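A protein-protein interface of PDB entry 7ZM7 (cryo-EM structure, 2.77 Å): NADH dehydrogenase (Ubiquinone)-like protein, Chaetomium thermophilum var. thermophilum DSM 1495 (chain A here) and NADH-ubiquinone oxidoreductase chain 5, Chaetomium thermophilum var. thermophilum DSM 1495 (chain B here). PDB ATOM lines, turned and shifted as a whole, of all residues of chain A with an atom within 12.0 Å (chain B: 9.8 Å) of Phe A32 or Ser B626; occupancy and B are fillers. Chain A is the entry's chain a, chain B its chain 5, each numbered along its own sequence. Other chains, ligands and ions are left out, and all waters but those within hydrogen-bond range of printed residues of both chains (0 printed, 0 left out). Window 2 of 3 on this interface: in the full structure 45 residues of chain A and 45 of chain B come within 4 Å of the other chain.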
ATOM      1  N   PHE A  32      27.707  23.201   9.818  1.00  0.00           N
ATOM      2  CA  PHE A  32      27.165  22.277   8.792  1.00  0.00           C
ATOM      3  C   PHE A  32      25.941  21.552   9.355  1.00  0.00           C
ATOM      4  O   PHE A  32      25.308  20.782   8.614  1.00  0.00           O
ATOM      5  CB  PHE A  32      28.211  21.239   8.380  1.00  0.00           C
ATOM      6  CG  PHE A  32      29.242  21.718   7.394  1.00  0.00           C
ATOM      7  CD1 PHE A  32      28.884  22.533   6.334  1.00  0.00           C
ATOM      8  CD2 PHE A  32      30.566  21.333   7.515  1.00  0.00           C
ATOM      9  CE1 PHE A  32      29.831  22.961   5.419  1.00  0.00           C
ATOM     10  CE2 PHE A  32      31.513  21.765   6.602  1.00  0.00           C
ATOM     11  CZ  PHE A  32      31.142  22.575   5.555  1.00  0.00           C
ATOM     12  N   LEU A  33      25.636  21.777  10.633  1.00  0.00           N
ATOM     13  CA  LEU A  33      24.524  21.030  11.263  1.00  0.00           C
ATOM     14  C   LEU A  33      23.206  21.829  11.263  1.00  0.00           C
ATOM     15  O   LEU A  33      23.279  23.064  11.298  1.00  0.00           O
ATOM     16  CB  LEU A  33      24.930  20.554  12.657  1.00  0.00           C
ATOM     17  CG  LEU A  33      25.753  19.267  12.682  1.00  0.00           C
ATOM     18  CD1 LEU A  33      26.144  18.900  14.102  1.00  0.00           C
ATOM     19  CD2 LEU A  33      24.988  18.125  12.034  1.00  0.00           C
ATOM     20  N   PRO A  34      22.007  21.187  11.217  1.00  0.00           N
ATOM     21  CA  PRO A  34      20.741  21.920  11.231  1.00  0.00           C
ATOM     22  C   PRO A  34      20.564  22.742  12.493  1.00  0.00           C
ATOM     23  O   PRO A  34      21.024  22.379  13.574  1.00  0.00           O
ATOM     24  CB  PRO A  34      19.693  20.811  11.142  1.00  0.00           C
ATOM     25  CG  PRO A  34      20.420  19.670  10.592  1.00  0.00           C
ATOM     26  CD  PRO A  34      21.788  19.741  11.098  1.00  0.00           C
ATOM     27  N   GLU A  35      19.871  23.865  12.332  1.00  0.00           N
ATOM     28  CA  GLU A  35      19.650  24.823  13.405  1.00  0.00           C
ATOM     29  C   GLU A  35      18.793  24.246  14.521  1.00  0.00           C
ATOM     30  O   GLU A  35      18.849  24.737  15.649  1.00  0.00           O
ATOM     31  CB  GLU A  35      19.016  26.078  12.803  1.00  0.00           C
ATOM     32  CG  GLU A  35      18.739  27.238  13.743  1.00  0.00           C
ATOM     33  CD  GLU A  35      19.998  27.849  14.320  1.00  0.00           C
ATOM     34  OE1 GLU A  35      21.063  27.739  13.678  1.00  0.00           O
ATOM     35  OE2 GLU A  35      19.913  28.468  15.401  1.00  0.00           O
ATOM     36  N   ALA A  36      18.009  23.212  14.237  1.00  0.00           N
ATOM     37  CA  ALA A  36      17.184  22.605  15.268  1.00  0.00           C
ATOM     38  C   ALA A  36      18.019  21.853  16.285  1.00  0.00           C
ATOM     39  O   ALA A  36      17.571  21.625  17.409  1.00  0.00           O
ATOM     40  CB  ALA A  36      16.177  21.669  14.625  1.00  0.00           C
ATOM     41  N   MET A  37      19.236  21.477  15.910  1.00  0.00           N
ATOM     42  CA  MET A  37      20.058  20.536  16.646  1.00  0.00           C
ATOM     43  C   MET A  37      21.158  21.206  17.446  1.00  0.00           C
ATOM     44  O   MET A  37      21.431  20.800  18.576  1.00  0.00           O
ATOM     45  CB  MET A  37      20.671  19.539  15.664  1.00  0.00           C
ATOM     46  CG  MET A  37      19.640  18.649  15.010  1.00  0.00           C
ATOM     47  SD  MET A  37      20.264  17.508  13.781  1.00  0.00           S
ATOM     48  CE  MET A  37      21.167  16.331  14.764  1.00  0.00           C
ATOM     49  N   VAL A  38      21.816  22.211  16.876  1.00  0.00           N
ATOM     50  CA  VAL A  38      22.861  22.962  17.559  1.00  0.00           C
ATOM     51  C   VAL A  38      22.467  24.406  17.794  1.00  0.00           C
ATOM     52  O   VAL A  38      23.165  25.117  18.520  1.00  0.00           O
ATOM     53  CB  VAL A  38      24.197  22.902  16.788  1.00  0.00           C
ATOM     54  CG1 VAL A  38      24.586  21.476  16.494  1.00  0.00           C
ATOM     55  CG2 VAL A  38      24.119  23.725  15.503  1.00  0.00           C
ATOM     56  N   GLY A  39      21.350  24.849  17.224  1.00  0.00           N
ATOM     57  CA  GLY A  39      21.024  26.262  17.258  1.00  0.00           C
ATOM     58  C   GLY A  39      20.752  26.763  18.665  1.00  0.00           C
ATOM     59  O   GLY A  39      20.144  26.077  19.486  1.00  0.00           O
ATOM     60  N   ARG A  40      21.180  27.990  18.964  1.00  0.00           N
ATOM     61  CA  ARG A  40      20.951  28.580  20.312  1.00  0.00           C
ATOM     62  C   ARG A  40      19.458  28.875  20.496  1.00  0.00           C
ATOM     63  O   ARG A  40      19.034  29.069  21.651  1.00  0.00           O
ATOM     64  CB  ARG A  40      21.820  29.838  20.440  1.00  0.00           C
ATOM     65  CG  ARG A  40      21.519  30.743  21.628  1.00  0.00           C
ATOM     66  CD  ARG A  40      21.902  30.196  22.993  1.00  0.00           C
ATOM     67  NE  ARG A  40      21.248  30.939  24.064  1.00  0.00           N
ATOM     68  CZ  ARG A  40      21.746  32.016  24.663  1.00  0.00           C
ATOM     69  NH1 ARG A  40      21.060  32.614  25.621  1.00  0.00           N
ATOM     70  NH2 ARG A  40      22.927  32.489  24.310  1.00  0.00           N
ATOM     71  N   SER A  41      18.669  28.823  19.420  1.00  0.00           N
ATOM     72  CA  SER A  41      17.280  29.242  19.521  1.00  0.00           C
ATOM     73  C   SER A  41      16.455  28.271  20.357  1.00  0.00           C
ATOM     74  O   SER A  41      15.715  28.689  21.252  1.00  0.00           O
ATOM     75  CB  SER A  41      16.694  29.384  18.118  1.00  0.00           C
ATOM     76  OG  SER A  41      17.561  30.143  17.294  1.00  0.00           O
ATOM     77  N   ILE A  43      17.315  26.354  22.637  1.00  0.00           N
ATOM     78  CA  ILE A  43      17.577  26.488  24.061  1.00  0.00           C
ATOM     79  C   ILE A  43      16.742  27.616  24.645  1.00  0.00           C
ATOM     80  O   ILE A  43      16.121  27.460  25.699  1.00  0.00           O
ATOM     81  CB  ILE A  43      19.081  26.650  24.319  1.00  0.00           C
ATOM     82  CG1 ILE A  43      19.815  25.388  23.869  1.00  0.00           C
ATOM     83  CG2 ILE A  43      19.343  26.864  25.765  1.00  0.00           C
ATOM     84  CD1 ILE A  43      20.253  25.363  22.451  1.00  0.00           C
ATOM     85  N   SER B 621      27.063  27.363  25.480  1.00  0.00           N
ATOM     86  CA  SER B 621      26.550  26.587  24.367  1.00  0.00           C
ATOM     87  C   SER B 621      26.190  27.450  23.167  1.00  0.00           C
ATOM     88  O   SER B 621      25.929  26.903  22.097  1.00  0.00           O
ATOM     89  CB  SER B 621      25.355  25.752  24.816  1.00  0.00           C
ATOM     90  OG  SER B 621      24.283  26.555  25.234  1.00  0.00           O
ATOM     91  N   SER B 622      26.185  28.773  23.310  1.00  0.00           N
ATOM     92  CA  SER B 622      26.100  29.653  22.151  1.00  0.00           C
ATOM     93  C   SER B 622      27.400  29.706  21.372  1.00  0.00           C
ATOM     94  O   SER B 622      27.428  30.280  20.282  1.00  0.00           O
ATOM     95  CB  SER B 622      25.716  31.068  22.578  1.00  0.00           C
ATOM     96  OG  SER B 622      26.791  31.730  23.222  1.00  0.00           O
ATOM     97  N   LEU B 623      28.476  29.158  21.919  1.00  0.00           N
ATOM     98  CA  LEU B 623      29.726  29.018  21.193  1.00  0.00           C
ATOM     99  C   LEU B 623      29.692  27.872  20.194  1.00  0.00           C
ATOM    100  O   LEU B 623      30.384  27.929  19.176  1.00  0.00           O
ATOM    101  CB  LEU B 623      30.868  28.811  22.185  1.00  0.00           C
ATOM    102  CG  LEU B 623      31.293  30.058  22.947  1.00  0.00           C
ATOM    103  CD1 LEU B 623      32.030  29.691  24.216  1.00  0.00           C
ATOM    104  CD2 LEU B 623      32.166  30.909  22.064  1.00  0.00           C
ATOM    105  N   SER B 624      28.910  26.834  20.463  1.00  0.00           N
ATOM    106  CA  SER B 624      28.975  25.579  19.713  1.00  0.00           C
ATOM    107  C   SER B 624      28.102  25.677  18.472  1.00  0.00           C
ATOM    108  O   SER B 624      26.890  25.493  18.538  1.00  0.00           O
ATOM    109  CB  SER B 624      28.541  24.419  20.600  1.00  0.00           C
ATOM    110  OG  SER B 624      29.495  24.185  21.617  1.00  0.00           O
ATOM    111  N   THR B 625      28.718  25.930  17.321  1.00  0.00           N
ATOM    112  CA  THR B 625      27.965  26.362  16.151  1.00  0.00           C
ATOM    113  C   THR B 625      28.045  25.353  15.004  1.00  0.00           C
ATOM    114  O   THR B 625      27.443  25.566  13.950  1.00  0.00           O
ATOM    115  CB  THR B 625      28.470  27.742  15.732  1.00  0.00           C
ATOM    116  OG1 THR B 625      28.289  28.639  16.828  1.00  0.00           O
ATOM    117  CG2 THR B 625      27.597  28.319  14.657  1.00  0.00           C
ATOM    118  N   SER B 626      28.731  24.230  15.213  1.00  0.00           N
ATOM    119  CA  SER B 626      28.962  23.212  14.191  1.00  0.00           C
ATOM    120  C   SER B 626      29.630  23.797  12.951  1.00  0.00           C
ATOM    121  O   SER B 626      29.388  23.348  11.833  1.00  0.00           O
ATOM    122  CB  SER B 626      27.673  22.486  13.813  1.00  0.00           C
ATOM    123  OG  SER B 626      26.879  23.284  12.971  1.00  0.00           O
ATOM    124  N   HIS B 627      30.498  24.792  13.166  1.00  0.00           N
ATOM    125  CA  HIS B 627      31.288  25.351  12.041  1.00  0.00           C
ATOM    126  C   HIS B 627      32.724  24.854  12.205  1.00  0.00           C
ATOM    127  O   HIS B 627      33.394  25.320  13.131  1.00  0.00           O
ATOM    128  CB  HIS B 627      31.184  26.878  11.981  1.00  0.00           C
ATOM    129  CG  HIS B 627      29.871  27.370  11.472  1.00  0.00           C
ATOM    130  ND1 HIS B 627      29.379  28.619  11.791  1.00  0.00           N
ATOM    131  CD2 HIS B 627      28.948  26.791  10.676  1.00  0.00           C
ATOM    132  CE1 HIS B 627      28.210  28.791  11.206  1.00  0.00           C
ATOM    133  NE2 HIS B 627      27.923  27.683  10.518  1.00  0.00           N
ATOM    134  N   VAL B 628      33.148  23.903  11.371  1.00  0.00           N
ATOM    135  CA  VAL B 628      34.488  23.348  11.477  1.00  0.00           C
ATOM    136  C   VAL B 628      35.533  24.444  11.459  1.00  0.00           C
ATOM    137  O   VAL B 628      36.550  24.350  12.149  1.00  0.00           O
ATOM    138  CB  VAL B 628      34.725  22.289  10.381  1.00  0.00           C
ATOM    139  CG1 VAL B 628      33.843  21.126  10.600  1.00  0.00           C
ATOM    140  CG2 VAL B 628      34.334  22.848   9.064  1.00  0.00           C
ATOM    141  N   THR B 629      35.298  25.504  10.696  1.00  0.00           N
ATOM    142  CA  THR B 629      36.264  26.588  10.640  1.00  0.00           C
ATOM    143  C   THR B 629      36.451  27.234  12.003  1.00  0.00           C
ATOM    144  O   THR B 629      37.582  27.518  12.407  1.00  0.00           O
ATOM    145  CB  THR B 629      35.826  27.617   9.602  1.00  0.00           C
ATOM    146  OG1 THR B 629      34.447  27.941   9.803  1.00  0.00           O
ATOM    147  CG2 THR B 629      36.016  27.074   8.206  1.00  0.00           C
ATOM    148  N   THR B 630      35.358  27.403  12.753  1.00  0.00           N
ATOM    149  CA  THR B 630      35.425  28.052  14.089  1.00  0.00           C
ATOM    150  C   THR B 630      35.996  27.071  15.123  1.00  0.00           C
ATOM    151  O   THR B 630      36.690  27.528  16.047  1.00  0.00           O
ATOM    152  CB  THR B 630      34.087  28.696  14.469  1.00  0.00           C
ATOM    153  OG1 THR B 630      33.186  27.707  14.963  1.00  0.00           O
ATOM    154  CG2 THR B 630      33.460  29.461  13.325  1.00  0.00           C
ATOM    155  N   TYR B 631      35.697  25.782  14.980  1.00  0.00           N
ATOM    156  CA  TYR B 631      36.215  24.759  15.922  1.00  0.00           C
ATOM    157  C   TYR B 631      37.734  24.684  15.839  1.00  0.00           C
ATOM    158  O   TYR B 631      38.376  24.549  16.882  1.00  0.00           O
ATOM    159  CB  TYR B 631      35.539  23.408  15.691  1.00  0.00           C
ATOM    160  CG  TYR B 631      34.122  23.319  16.197  1.00  0.00           C
ATOM    161  CD1 TYR B 631      33.558  24.344  16.940  1.00  0.00           C
ATOM    162  CD2 TYR B 631      33.343  22.206  15.942  1.00  0.00           C
ATOM    163  CE1 TYR B 631      32.256  24.270  17.406  1.00  0.00           C
ATOM    164  CE2 TYR B 631      32.041  22.112  16.400  1.00  0.00           C
ATOM    165  CZ  TYR B 631      31.496  23.147  17.137  1.00  0.00           C
ATOM    166  OH  TYR B 631      30.214  23.055  17.592  1.00  0.00           O
ATOM    167  N   ALA B 632      38.280  24.766  14.637  1.00  0.00           N
ATOM    168  CA  ALA B 632      39.736  24.671  14.433  1.00  0.00           C
ATOM    169  C   ALA B 632      40.437  25.816  15.157  1.00  0.00           C
ATOM    170  O   ALA B 632      41.478  25.569  15.795  1.00  0.00           O
ATOM    171  CB  ALA B 632      39.976  24.765  12.964  1.00  0.00           C
ATOM    172  N   TYR B 634      39.339  27.401  17.734  1.00  0.00           N
ATOM    173  CA  TYR B 634      39.206  27.176  19.196  1.00  0.00           C
ATOM    174  C   TYR B 634      40.282  26.200  19.679  1.00  0.00           C
ATOM    175  O   TYR B 634      40.828  26.417  20.768  1.00  0.00           O
ATOM    176  CB  TYR B 634      37.825  26.621  19.562  1.00  0.00           C
ATOM    177  CG  TYR B 634      36.634  27.526  19.401  1.00  0.00           C
ATOM    178  CD1 TYR B 634      36.767  28.900  19.297  1.00  0.00           C
ATOM    179  CD2 TYR B 634      35.356  26.995  19.377  1.00  0.00           C
ATOM    180  CE1 TYR B 634      35.659  29.719  19.159  1.00  0.00           C
ATOM    181  CE2 TYR B 634      34.238  27.800  19.244  1.00  0.00           C
ATOM    182  CZ  TYR B 634      34.392  29.167  19.132  1.00  0.00           C
ATOM    183  OH  TYR B 634      33.297  29.966  18.990  1.00  0.00           O
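Hydrophobic or aromatic side chains of chain A that line the printed part of chain B: Phe A32, Leu A33 and Val A38. Of the 13 printed residues of chain B, 5 touch a printed residue of chain A. Among the printed residues, 7 pairs touch across the chains.
Phe A32 touches three residues of chain B. Of the printed residues of chain B, Arg A40 touches Ser B622. Ser A41 touches none of the printed residues of chain B. Of the printed residues of chain A, Ser B622 touches Arg A40. Of the printed residues of chain A, Ser B624 touches Val A38. Ser B626 touches just these residues of chain A: Phe A32, Leu A33 and Val A38. Val B628 touches just one residue of chain A: Phe A32. Tyr B631 touches none of the printed residues of chain A. The nearest residue of chain B that does not touch Phe A32 is Thr B625 (4.8 Å). The nearest residue of chain A that does not touch Ser B626 is Pro A34 (5.6 Å). The nearest printed residue of chain A that does not touch Ser B622 is Val A38 (6.5 Å).
The backbone carbonyl oxygen (O) of Ser B626 is in hydrogen-bond range of the backbone NH (N) of Phe A32, at 2.6 Å. N of Leu A33 sits at hydrogen-bond distance from OG of Ser B626 (3.0 Å).
CD2 of His B627 touches N of Phe A32 (3.9 Å). CG2 of Val B628 touches CE2 of Phe A32, 3.9 Å away. O of Val A38 touches O of Ser B624, 3.7 Å away. Ser B626 touches Val A38 (OG to CG2, 3.8 Å). Ser B622 touches Arg A40.
The side-chain hydroxyl (OH) of Tyr B631 sits at hydrogen-bond distance from the backbone NH (N) of Ser B626, 3.0 Å away. O of His B627 sits at hydrogen-bond distance from OG1 of Thr B630 (3.0 Å).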
